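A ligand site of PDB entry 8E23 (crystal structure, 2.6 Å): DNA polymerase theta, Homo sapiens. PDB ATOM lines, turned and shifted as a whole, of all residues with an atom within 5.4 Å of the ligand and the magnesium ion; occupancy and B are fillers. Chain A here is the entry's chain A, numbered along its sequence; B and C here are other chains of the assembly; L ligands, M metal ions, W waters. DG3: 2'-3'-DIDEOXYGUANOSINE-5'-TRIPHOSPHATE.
O2B of the ligand lies close to O of Ser 418 (3.0 Å).
O6 of DG 13 of chain C sits close to an oxygen (O6) of the ligand.
NE2 of Gln 419 touches O2G of the ligand, at 3.7 Å.
Glu 421 touches the ligand (CD to C2', 3.5 Å).
CZ of Phe 445 touches O1B of the ligand (3.3 Å).
Gln 470 touches the ligand (CG to O6, 3.8 Å).
Tyr 477 touches the ligand.
Hydrophobic or aromatic side chains that line the ligand: Phe 445, Tyr 473 and Tyr 477.
The nearest printed residue that does not touch the ligand is Tyr 417 (4.04 Å).
NH2 of Arg 367 is in hydrogen-bond range of O4' of the ligand.
N1 of DC 5 of chain B lies close to a nitrogen (N2) of the ligand, 3.4 Å away.
N3 of DC 4 of chain B is in hydrogen-bond range of a nitrogen (N1) of the ligand (2.6 Å).
NH2 of Arg 465 lies within salt-bridge range of O2G of the ligand (2.9 Å).
OH of Tyr 473 is in hydrogen-bond range of O1B of the ligand, 2.5 Å away.
NZ of Lys 469 is in salt-bridge range of O3G of the ligand (2.6 Å).
O1G of the ligand binds the magnesium ion (2.1 Å).
OD2 of Asp 618 is bound to the magnesium ion (2.1 Å).
The magnesium ion is bound by water W1.
O2A of the ligand binds the magnesium ion (2.2 Å).
The magnesium ion is bound by O2B of the ligand, at 2.3 Å.
Merely in contact with the magnesium ion: Tyr 417 (3.3 Å), Asp 416 (3.8 Å) and Ser 418 (3.8 Å).
Within 4 Å of the magnesium ion: Asp 416, Tyr 417, Ser 418 and Asp 618.
N4 of DC 4 of chain B is in hydrogen-bond range of NE2 of Gln 470.
O2 of DC 5 of chain B lies close to N2 of DG 13 of chain C, at 2.6 Å.
N2 of DG 13 of chain C lies within hydrogen-bond range of NE2 of Gln 560 (3.4 Å).
The guanidinium group (NH2) of Arg 465 lies within salt-bridge range of the side-chain carboxylate (OD2) of Asp 443, at 2.6 Å.
OE2 of Glu 421 lies within salt-bridge range of NH2 of Arg 367 (3.3 Å).
The backbone NH (N) of Phe 445 sits at hydrogen-bond distance from the side-chain carboxylate (OD1) of Asp 443 (2.7 Å).
The backbone carbonyl oxygen (O) of Asp 618 lies within hydrogen-bond range of the backbone NH (N) of Tyr 417, at 3.0 Å.
NE2 of Gln 560 lies within hydrogen-bond range of O2 of DC 5 of chain B, 3.3 Å away.
Water W1 lies within hydrogen-bond range of the side-chain carboxylate (OD2) of Asp 416 (3.0 Å) and the side-chain carboxylate (OD1) of Asp 618 (3.5 Å).
Water W3 bridges the side-chain amide nitrogen of Gln 466 (2.5 Å) and an oxygen (O1A) of the ligand (2.8 Å).
Water W2 lies within hydrogen-bond range of the side-chain amide nitrogen (NE2) of Gln 560 (2.6 Å), the side-chain amide nitrogen (ND2) of Asn 556 (2.8 Å), the side-chain carboxylate (OE1) of Glu 421 (2.9 Å) and a nitrogen (N3) of the ligand (3.2 Å).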
ATOM      1  N   ARG A 367      11.331 -35.752  21.771  1.00  0.00           N
ATOM      2  CA  ARG A 367      10.729 -34.887  20.768  1.00  0.00           C
ATOM      3  C   ARG A 367      10.058 -35.716  19.682  1.00  0.00           C
ATOM      4  O   ARG A 367      10.278 -36.925  19.548  1.00  0.00           O
ATOM      5  CB  ARG A 367      11.773 -33.952  20.156  1.00  0.00           C
ATOM      6  CG  ARG A 367      12.167 -32.785  21.029  1.00  0.00           C
ATOM      7  CD  ARG A 367      13.027 -31.803  20.245  1.00  0.00           C
ATOM      8  NE  ARG A 367      13.170 -30.522  20.900  1.00  0.00           N
ATOM      9  CZ  ARG A 367      13.646 -29.427  20.322  1.00  0.00           C
ATOM     10  NH1 ARG A 367      14.033 -29.432  19.055  1.00  0.00           N
ATOM     11  NH2 ARG A 367      13.742 -28.302  21.025  1.00  0.00           N
ATOM     12  N   ASP A 416       2.113 -21.573  20.309  1.00  0.00           N
ATOM     13  CA  ASP A 416       3.429 -21.987  20.755  1.00  0.00           C
ATOM     14  C   ASP A 416       3.702 -21.465  22.151  1.00  0.00           C
ATOM     15  O   ASP A 416       3.287 -20.361  22.509  1.00  0.00           O
ATOM     16  CB  ASP A 416       4.516 -21.479  19.791  1.00  0.00           C
ATOM     17  CG  ASP A 416       4.453 -19.979  19.566  1.00  0.00           C
ATOM     18  OD1 ASP A 416       3.333 -19.435  19.510  1.00  0.00           O
ATOM     19  OD2 ASP A 416       5.524 -19.351  19.438  1.00  0.00           O
ATOM     20  N   TYR A 417       4.405 -22.274  22.939  1.00  0.00           N
ATOM     21  CA  TYR A 417       4.946 -21.789  24.199  1.00  0.00           C
ATOM     22  C   TYR A 417       6.030 -20.753  23.922  1.00  0.00           C
ATOM     23  O   TYR A 417       6.850 -20.926  23.016  1.00  0.00           O
ATOM     24  CB  TYR A 417       5.512 -22.942  25.032  1.00  0.00           C
ATOM     25  CG  TYR A 417       4.475 -23.903  25.559  1.00  0.00           C
ATOM     26  CD1 TYR A 417       3.662 -23.558  26.639  1.00  0.00           C
ATOM     27  CD2 TYR A 417       4.315 -25.165  25.004  1.00  0.00           C
ATOM     28  CE1 TYR A 417       2.713 -24.436  27.132  1.00  0.00           C
ATOM     29  CE2 TYR A 417       3.370 -26.052  25.495  1.00  0.00           C
ATOM     30  CZ  TYR A 417       2.575 -25.684  26.558  1.00  0.00           C
ATOM     31  OH  TYR A 417       1.639 -26.556  27.049  1.00  0.00           O
ATOM     32  N   SER A 418       6.027 -19.666  24.688  1.00  0.00           N
ATOM     33  CA  SER A 418       6.922 -18.555  24.424  1.00  0.00           C
ATOM     34  C   SER A 418       8.385 -18.979  24.537  1.00  0.00           C
ATOM     35  O   SER A 418       9.136 -18.934  23.557  1.00  0.00           O
ATOM     36  CB  SER A 418       6.627 -17.397  25.378  1.00  0.00           C
ATOM     37  OG  SER A 418       5.333 -16.864  25.127  1.00  0.00           O
ATOM     38  N   GLN A 419       8.807 -19.395  25.736  1.00  0.00           N
ATOM     39  CA  GLN A 419      10.159 -19.920  25.975  1.00  0.00           C
ATOM     40  C   GLN A 419      10.020 -21.098  26.935  1.00  0.00           C
ATOM     41  O   GLN A 419      10.318 -20.996  28.121  1.00  0.00           O
ATOM     42  CB  GLN A 419      11.110 -18.852  26.524  1.00  0.00           C
ATOM     43  CG  GLN A 419      11.548 -17.810  25.498  1.00  0.00           C
ATOM     44  CD  GLN A 419      10.566 -16.659  25.385  1.00  0.00           C
ATOM     45  OE1 GLN A 419       9.665 -16.511  26.219  1.00  0.00           O
ATOM     46  NE2 GLN A 419      10.731 -15.838  24.357  1.00  0.00           N
ATOM     47  N   LEU A 420       9.551 -22.233  26.410  1.00  0.00           N
ATOM     48  CA  LEU A 420       9.221 -23.379  27.250  1.00  0.00           C
ATOM     49  C   LEU A 420      10.456 -23.918  27.964  1.00  0.00           C
ATOM     50  O   LEU A 420      10.403 -24.223  29.164  1.00  0.00           O
ATOM     51  CB  LEU A 420       8.565 -24.476  26.420  1.00  0.00           C
ATOM     52  CG  LEU A 420       8.017 -25.671  27.210  1.00  0.00           C
ATOM     53  CD1 LEU A 420       7.084 -25.195  28.306  1.00  0.00           C
ATOM     54  CD2 LEU A 420       7.307 -26.651  26.280  1.00  0.00           C
ATOM     55  N   GLU A 421      11.577 -24.062  27.248  1.00  0.00           N
ATOM     56  CA  GLU A 421      12.770 -24.614  27.869  1.00  0.00           C
ATOM     57  C   GLU A 421      13.403 -23.649  28.859  1.00  0.00           C
ATOM     58  O   GLU A 421      14.021 -24.086  29.838  1.00  0.00           O
ATOM     59  CB  GLU A 421      13.783 -25.033  26.796  1.00  0.00           C
ATOM     60  CG  GLU A 421      13.317 -26.206  25.954  1.00  0.00           C
ATOM     61  CD  GLU A 421      14.424 -26.818  25.119  1.00  0.00           C
ATOM     62  OE1 GLU A 421      15.607 -26.518  25.388  1.00  0.00           O
ATOM     63  OE2 GLU A 421      14.118 -27.595  24.196  1.00  0.00           O
ATOM     64  N   ASP A 443      11.329  -9.483  26.201  1.00  0.00           N
ATOM     65  CA  ASP A 443      11.921 -10.615  25.495  1.00  0.00           C
ATOM     66  C   ASP A 443      13.368 -10.805  25.923  1.00  0.00           C
ATOM     67  O   ASP A 443      14.175  -9.876  25.859  1.00  0.00           O
ATOM     68  CB  ASP A 443      11.833 -10.394  23.984  1.00  0.00           C
ATOM     69  CG  ASP A 443      12.195 -11.629  23.183  1.00  0.00           C
ATOM     70  OD1 ASP A 443      13.335 -12.109  23.306  1.00  0.00           O
ATOM     71  OD2 ASP A 443      11.326 -12.138  22.447  1.00  0.00           O
ATOM     72  N   PHE A 445      15.689 -12.739  24.517  1.00  0.00           N
ATOM     73  CA  PHE A 445      16.621 -12.737  23.397  1.00  0.00           C
ATOM     74  C   PHE A 445      16.909 -11.321  22.912  1.00  0.00           C
ATOM     75  O   PHE A 445      18.057 -10.989  22.587  1.00  0.00           O
ATOM     76  CB  PHE A 445      16.077 -13.596  22.258  1.00  0.00           C
ATOM     77  CG  PHE A 445      15.767 -15.008  22.670  1.00  0.00           C
ATOM     78  CD1 PHE A 445      16.544 -15.655  23.616  1.00  0.00           C
ATOM     79  CD2 PHE A 445      14.706 -15.698  22.099  1.00  0.00           C
ATOM     80  CE1 PHE A 445      16.259 -16.958  23.995  1.00  0.00           C
ATOM     81  CE2 PHE A 445      14.426 -16.997  22.470  1.00  0.00           C
ATOM     82  CZ  PHE A 445      15.202 -17.623  23.425  1.00  0.00           C
ATOM     83  N   ARG A 465      17.886 -11.345  16.687  1.00  0.00           N
ATOM     84  CA  ARG A 465      17.232 -12.053  17.784  1.00  0.00           C
ATOM     85  C   ARG A 465      17.443 -13.551  17.670  1.00  0.00           C
ATOM     86  O   ARG A 465      17.642 -14.241  18.685  1.00  0.00           O
ATOM     87  CB  ARG A 465      15.736 -11.725  17.793  1.00  0.00           C
ATOM     88  CG  ARG A 465      14.964 -12.396  18.927  1.00  0.00           C
ATOM     89  CD  ARG A 465      13.480 -12.062  18.883  1.00  0.00           C
ATOM     90  NE  ARG A 465      12.755 -12.660  19.990  1.00  0.00           N
ATOM     91  CZ  ARG A 465      12.185 -13.863  19.962  1.00  0.00           C
ATOM     92  NH1 ARG A 465      12.239 -14.615  18.873  1.00  0.00           N
ATOM     93  NH2 ARG A 465      11.560 -14.306  21.039  1.00  0.00           N
ATOM     94  N   GLN A 466      17.419 -14.089  16.449  1.00  0.00           N
ATOM     95  CA  GLN A 466      17.709 -15.501  16.260  1.00  0.00           C
ATOM     96  C   GLN A 466      19.160 -15.827  16.588  1.00  0.00           C
ATOM     97  O   GLN A 466      19.451 -16.923  17.088  1.00  0.00           O
ATOM     98  CB  GLN A 466      17.381 -15.916  14.820  1.00  0.00           C
ATOM     99  CG  GLN A 466      17.151 -17.410  14.639  1.00  0.00           C
ATOM    100  CD  GLN A 466      15.801 -17.864  15.150  1.00  0.00           C
ATOM    101  OE1 GLN A 466      15.012 -17.059  15.661  1.00  0.00           O
ATOM    102  NE2 GLN A 466      15.514 -19.143  15.000  1.00  0.00           N
ATOM    103  N   LYS A 469      19.319 -15.839  20.254  1.00  0.00           N
ATOM    104  CA  LYS A 469      18.666 -17.059  20.745  1.00  0.00           C
ATOM    105  C   LYS A 469      19.655 -18.222  20.768  1.00  0.00           C
ATOM    106  O   LYS A 469      19.686 -18.994  21.734  1.00  0.00           O
ATOM    107  CB  LYS A 469      17.470 -17.392  19.864  1.00  0.00           C
ATOM    108  CG  LYS A 469      16.832 -18.737  20.166  1.00  0.00           C
ATOM    109  CD  LYS A 469      15.784 -19.101  19.119  1.00  0.00           C
ATOM    110  CE  LYS A 469      14.708 -18.025  19.042  1.00  0.00           C
ATOM    111  NZ  LYS A 469      13.688 -18.345  18.007  1.00  0.00           N
ATOM    112  N   GLN A 470      20.457 -18.364  19.717  1.00  0.00           N
ATOM    113  CA  GLN A 470      21.435 -19.451  19.670  1.00  0.00           C
ATOM    114  C   GLN A 470      22.507 -19.270  20.732  1.00  0.00           C
ATOM    115  O   GLN A 470      22.993 -20.251  21.300  1.00  0.00           O
ATOM    116  CB  GLN A 470      22.052 -19.525  18.280  1.00  0.00           C
ATOM    117  CG  GLN A 470      23.028 -20.675  18.090  1.00  0.00           C
ATOM    118  CD  GLN A 470      23.454 -20.852  16.640  1.00  0.00           C
ATOM    119  OE1 GLN A 470      23.043 -20.090  15.774  1.00  0.00           O
ATOM    120  NE2 GLN A 470      24.287 -21.855  16.386  1.00  0.00           N
ATOM    121  N   TYR A 473      20.742 -20.283  24.402  1.00  0.00           N
ATOM    122  CA  TYR A 473      20.683 -21.726  24.608  1.00  0.00           C
ATOM    123  C   TYR A 473      22.052 -22.368  24.512  1.00  0.00           C
ATOM    124  O   TYR A 473      22.318 -23.373  25.178  1.00  0.00           O
ATOM    125  CB  TYR A 473      19.719 -22.363  23.605  1.00  0.00           C
ATOM    126  CG  TYR A 473      18.266 -22.017  23.861  1.00  0.00           C
ATOM    127  CD1 TYR A 473      17.632 -22.446  25.014  1.00  0.00           C
ATOM    128  CD2 TYR A 473      17.552 -21.258  22.954  1.00  0.00           C
ATOM    129  CE1 TYR A 473      16.315 -22.133  25.258  1.00  0.00           C
ATOM    130  CE2 TYR A 473      16.215 -20.942  23.189  1.00  0.00           C
ATOM    131  CZ  TYR A 473      15.609 -21.380  24.342  1.00  0.00           C
ATOM    132  OH  TYR A 473      14.288 -21.059  24.587  1.00  0.00           O
ATOM    133  N   GLY A 474      22.952 -21.801  23.704  1.00  0.00           N
ATOM    134  CA  GLY A 474      24.302 -22.343  23.622  1.00  0.00           C
ATOM    135  C   GLY A 474      25.023 -22.259  24.958  1.00  0.00           C
ATOM    136  O   GLY A 474      25.599 -23.246  25.425  1.00  0.00           O
ATOM    137  N   TYR A 477      23.617 -24.634  27.714  1.00  0.00           N
ATOM    138  CA  TYR A 477      23.937 -26.048  27.554  1.00  0.00           C
ATOM    139  C   TYR A 477      25.422 -26.298  27.350  1.00  0.00           C
ATOM    140  O   TYR A 477      25.801 -27.319  26.760  1.00  0.00           O
ATOM    141  CB  TYR A 477      23.119 -26.630  26.399  1.00  0.00           C
ATOM    142  CG  TYR A 477      21.620 -26.561  26.634  1.00  0.00           C
ATOM    143  CD1 TYR A 477      21.050 -27.164  27.742  1.00  0.00           C
ATOM    144  CD2 TYR A 477      20.793 -25.893  25.744  1.00  0.00           C
ATOM    145  CE1 TYR A 477      19.683 -27.107  27.961  1.00  0.00           C
ATOM    146  CE2 TYR A 477      19.427 -25.824  25.956  1.00  0.00           C
ATOM    147  CZ  TYR A 477      18.882 -26.427  27.066  1.00  0.00           C
ATOM    148  OH  TYR A 477      17.520 -26.366  27.277  1.00  0.00           O
ATOM    149  N   ASN A 556      20.699 -31.037  28.950  1.00  0.00           N
ATOM    150  CA  ASN A 556      19.745 -30.765  27.872  1.00  0.00           C
ATOM    151  C   ASN A 556      18.586 -31.763  27.886  1.00  0.00           C
ATOM    152  O   ASN A 556      17.441 -31.382  27.624  1.00  0.00           O
ATOM    153  CB  ASN A 556      20.462 -30.799  26.522  1.00  0.00           C
ATOM    154  CG  ASN A 556      19.515 -30.606  25.348  1.00  0.00           C
ATOM    155  OD1 ASN A 556      19.056 -31.573  24.734  1.00  0.00           O
ATOM    156  ND2 ASN A 556      19.214 -29.348  25.032  1.00  0.00           N
ATOM    157  N   GLN A 560      15.028 -30.177  27.641  1.00  0.00           N
ATOM    158  CA  GLN A 560      14.378 -30.427  26.354  1.00  0.00           C
ATOM    159  C   GLN A 560      13.411 -31.604  26.432  1.00  0.00           C
ATOM    160  O   GLN A 560      12.383 -31.614  25.754  1.00  0.00           O
ATOM    161  CB  GLN A 560      15.439 -30.676  25.278  1.00  0.00           C
ATOM    162  CG  GLN A 560      14.883 -30.837  23.876  1.00  0.00           C
ATOM    163  CD  GLN A 560      15.944 -31.247  22.874  1.00  0.00           C
ATOM    164  OE1 GLN A 560      15.906 -32.351  22.327  1.00  0.00           O
ATOM    165  NE2 GLN A 560      16.900 -30.357  22.627  1.00  0.00           N
ATOM    166  N   ASP A 618       7.855 -26.946  20.165  1.00  0.00           N
ATOM    167  CA  ASP A 618       7.203 -26.087  21.144  1.00  0.00           C
ATOM    168  C   ASP A 618       5.978 -25.379  20.566  1.00  0.00           C
ATOM    169  O   ASP A 618       5.432 -24.483  21.211  1.00  0.00           O
ATOM    170  CB  ASP A 618       8.189 -25.063  21.717  1.00  0.00           C
ATOM    171  CG  ASP A 618       8.493 -23.927  20.745  1.00  0.00           C
ATOM    172  OD1 ASP A 618       8.460 -24.153  19.518  1.00  0.00           O
ATOM    173  OD2 ASP A 618       8.761 -22.811  21.219  1.00  0.00           O
ATOM    174  P    DC B   4      31.320 -26.287  22.122  1.00  0.00           P
ATOM    175  OP1  DC B   4      31.364 -26.036  20.664  1.00  0.00           O
ATOM    176  OP2  DC B   4      32.089 -25.423  23.043  1.00  0.00           O
ATOM    177  O5'  DC B   4      29.787 -26.270  22.600  1.00  0.00           O
ATOM    178  C5'  DC B   4      28.895 -27.275  22.152  1.00  0.00           C
ATOM    179  C4'  DC B   4      27.664 -27.328  23.036  1.00  0.00           C
ATOM    180  O4'  DC B   4      26.991 -26.054  22.987  1.00  0.00           O
ATOM    181  C3'  DC B   4      26.618 -28.355  22.614  1.00  0.00           C
ATOM    182  O3'  DC B   4      26.908 -29.617  23.209  1.00  0.00           O
ATOM    183  C2'  DC B   4      25.338 -27.751  23.181  1.00  0.00           C
ATOM    184  C1'  DC B   4      25.590 -26.245  23.068  1.00  0.00           C
ATOM    185  N1   DC B   4      24.964 -25.622  21.860  1.00  0.00           N
ATOM    186  C2   DC B   4      23.587 -25.358  21.859  1.00  0.00           C
ATOM    187  O2   DC B   4      22.910 -25.664  22.857  1.00  0.00           O
ATOM    188  N3   DC B   4      23.026 -24.792  20.762  1.00  0.00           N
ATOM    189  C4   DC B   4      23.789 -24.481  19.715  1.00  0.00           C
ATOM    190  N4   DC B   4      23.188 -23.919  18.656  1.00  0.00           N
ATOM    191  C5   DC B   4      25.187 -24.731  19.698  1.00  0.00           C
ATOM    192  C6   DC B   4      25.728 -25.293  20.785  1.00  0.00           C
ATOM    193  P    DC B   5      26.716 -30.975  22.376  1.00  0.00           P
ATOM    194  OP1  DC B   5      27.357 -32.066  23.132  1.00  0.00           O
ATOM    195  OP2  DC B   5      27.119 -30.699  20.978  1.00  0.00           O
ATOM    196  O5'  DC B   5      25.131 -31.209  22.392  1.00  0.00           O
ATOM    197  C5'  DC B   5      24.462 -31.453  23.613  1.00  0.00           C
ATOM    198  C4'  DC B   5      22.961 -31.383  23.434  1.00  0.00           C
ATOM    199  O4'  DC B   5      22.578 -30.037  23.100  1.00  0.00           O
ATOM    200  C3'  DC B   5      22.403 -32.229  22.306  1.00  0.00           C
ATOM    201  O3'  DC B   5      22.196 -33.564  22.752  1.00  0.00           O
ATOM    202  C2'  DC B   5      21.080 -31.531  22.004  1.00  0.00           C
ATOM    203  C1'  DC B   5      21.387 -30.061  22.319  1.00  0.00           C
ATOM    204  N1   DC B   5      21.595 -29.216  21.102  1.00  0.00           N
ATOM    205  C2   DC B   5      20.484 -28.783  20.372  1.00  0.00           C
ATOM    206  O2   DC B   5      19.352 -29.096  20.753  1.00  0.00           O
ATOM    207  N3   DC B   5      20.679 -28.013  19.276  1.00  0.00           N
ATOM    208  C4   DC B   5      21.913 -27.696  18.894  1.00  0.00           C
ATOM    209  N4   DC B   5      22.059 -26.939  17.801  1.00  0.00           N
ATOM    210  C5   DC B   5      23.065 -28.131  19.622  1.00  0.00           C
ATOM    211  C6   DC B   5      22.862 -28.891  20.707  1.00  0.00           C
ATOM    212  P    DG C  13      12.500 -22.554  13.022  1.00  0.00           P
ATOM    213  OP1  DG C  13      11.288 -21.707  12.919  1.00  0.00           O
ATOM    214  OP2  DG C  13      13.838 -21.928  12.987  1.00  0.00           O
ATOM    215  O5'  DG C  13      12.418 -23.430  14.360  1.00  0.00           O
ATOM    216  C5'  DG C  13      11.274 -24.238  14.598  1.00  0.00           C
ATOM    217  C4'  DG C  13      11.530 -25.209  15.750  1.00  0.00           C
ATOM    218  O4'  DG C  13      12.638 -26.067  15.425  1.00  0.00           O
ATOM    219  C3'  DG C  13      11.915 -24.560  17.059  1.00  0.00           C
ATOM    220  C2'  DG C  13      12.629 -25.698  17.773  1.00  0.00           C
ATOM    221  C1'  DG C  13      13.331 -26.418  16.613  1.00  0.00           C
ATOM    222  N9   DG C  13      14.735 -26.067  16.472  1.00  0.00           N
ATOM    223  C8   DG C  13      15.290 -25.214  15.549  1.00  0.00           C
ATOM    224  N7   DG C  13      16.575 -25.092  15.656  1.00  0.00           N
ATOM    225  C5   DG C  13      16.910 -25.918  16.723  1.00  0.00           C
ATOM    226  C6   DG C  13      18.171 -26.206  17.308  1.00  0.00           C
ATOM    227  O6   DG C  13      19.277 -25.747  16.983  1.00  0.00           O
ATOM    228  N1   DG C  13      18.061 -27.095  18.361  1.00  0.00           N
ATOM    229  C2   DG C  13      16.881 -27.656  18.795  1.00  0.00           C
ATOM    230  N2   DG C  13      16.973 -28.503  19.835  1.00  0.00           N
ATOM    231  N3   DG C  13      15.695 -27.399  18.263  1.00  0.00           N
ATOM    232  C4   DG C  13      15.787 -26.532  17.227  1.00  0.00           C
HETATM  233  PG  DG3 L   1      10.516 -17.891  20.289  1.00  0.00           P
HETATM  234  O1G DG3 L   1       9.536 -19.031  20.090  1.00  0.00           O
HETATM  235  O2G DG3 L   1       9.894 -16.650  20.881  1.00  0.00           O
HETATM  236  O3G DG3 L   1      11.396 -17.641  19.095  1.00  0.00           O
HETATM  237  O3B DG3 L   1      11.528 -18.395  21.428  1.00  0.00           O
HETATM  238  PB  DG3 L   1      11.927 -19.947  21.587  1.00  0.00           P
HETATM  239  O1B DG3 L   1      13.027 -20.029  22.627  1.00  0.00           O
HETATM  240  O2B DG3 L   1      10.693 -20.780  21.785  1.00  0.00           O
HETATM  241  O3A DG3 L   1      12.594 -20.258  20.151  1.00  0.00           O
HETATM  242  PA  DG3 L   1      12.183 -21.559  19.292  1.00  0.00           P
HETATM  243  O1A DG3 L   1      12.925 -21.474  17.976  1.00  0.00           O
HETATM  244  O2A DG3 L   1      10.682 -21.726  19.289  1.00  0.00           O
HETATM  245  O5' DG3 L   1      12.844 -22.742  20.167  1.00  0.00           O
HETATM  246  C5' DG3 L   1      12.048 -23.814  20.645  1.00  0.00           C
HETATM  247  C4' DG3 L   1      12.920 -24.731  21.481  1.00  0.00           C
HETATM  248  O4' DG3 L   1      14.007 -25.226  20.690  1.00  0.00           O
HETATM  249  C3' DG3 L   1      13.534 -23.941  22.627  1.00  0.00           C
HETATM  250  C2' DG3 L   1      14.984 -24.386  22.697  1.00  0.00           C
HETATM  251  C1' DG3 L   1      15.226 -25.218  21.442  1.00  0.00           C
HETATM  252  N9  DG3 L   1      16.312 -24.587  20.649  1.00  0.00           N
HETATM  253  C8  DG3 L   1      16.149 -23.713  19.642  1.00  0.00           C
HETATM  254  N7  DG3 L   1      17.360 -23.336  19.126  1.00  0.00           N
HETATM  255  C5  DG3 L   1      18.310 -23.985  19.822  1.00  0.00           C
HETATM  256  C6  DG3 L   1      19.790 -24.050  19.803  1.00  0.00           C
HETATM  257  O6  DG3 L   1      20.449 -23.381  18.979  1.00  0.00           O
HETATM  258  N1  DG3 L   1      20.392 -24.847  20.689  1.00  0.00           N
HETATM  259  C2  DG3 L   1      19.708 -25.585  21.578  1.00  0.00           C
HETATM  260  N2  DG3 L   1      20.397 -26.371  22.445  1.00  0.00           N
HETATM  261  N3  DG3 L   1      18.355 -25.574  21.658  1.00  0.00           N
HETATM  262  C4  DG3 L   1      17.615 -24.806  20.816  1.00  0.00           C
HETATM  263 MG    MG M   1       8.854 -20.951  20.344  1.00  0.00          MG
HETATM  264  O   HOH W   1       7.916 -20.902  18.493  1.00  0.00           O
HETATM  265  O   HOH W   2      17.265 -27.944  23.500  1.00  0.00           O
HETATM  266  O   HOH W   3      15.236 -21.276  16.352  1.00  0.00           O
HETATM  267  O   HOH W   4       9.281 -21.406  16.359  1.00  0.00           O
HETATM  268  O   HOH W   5      10.092 -22.677  24.074  1.00  0.00           O
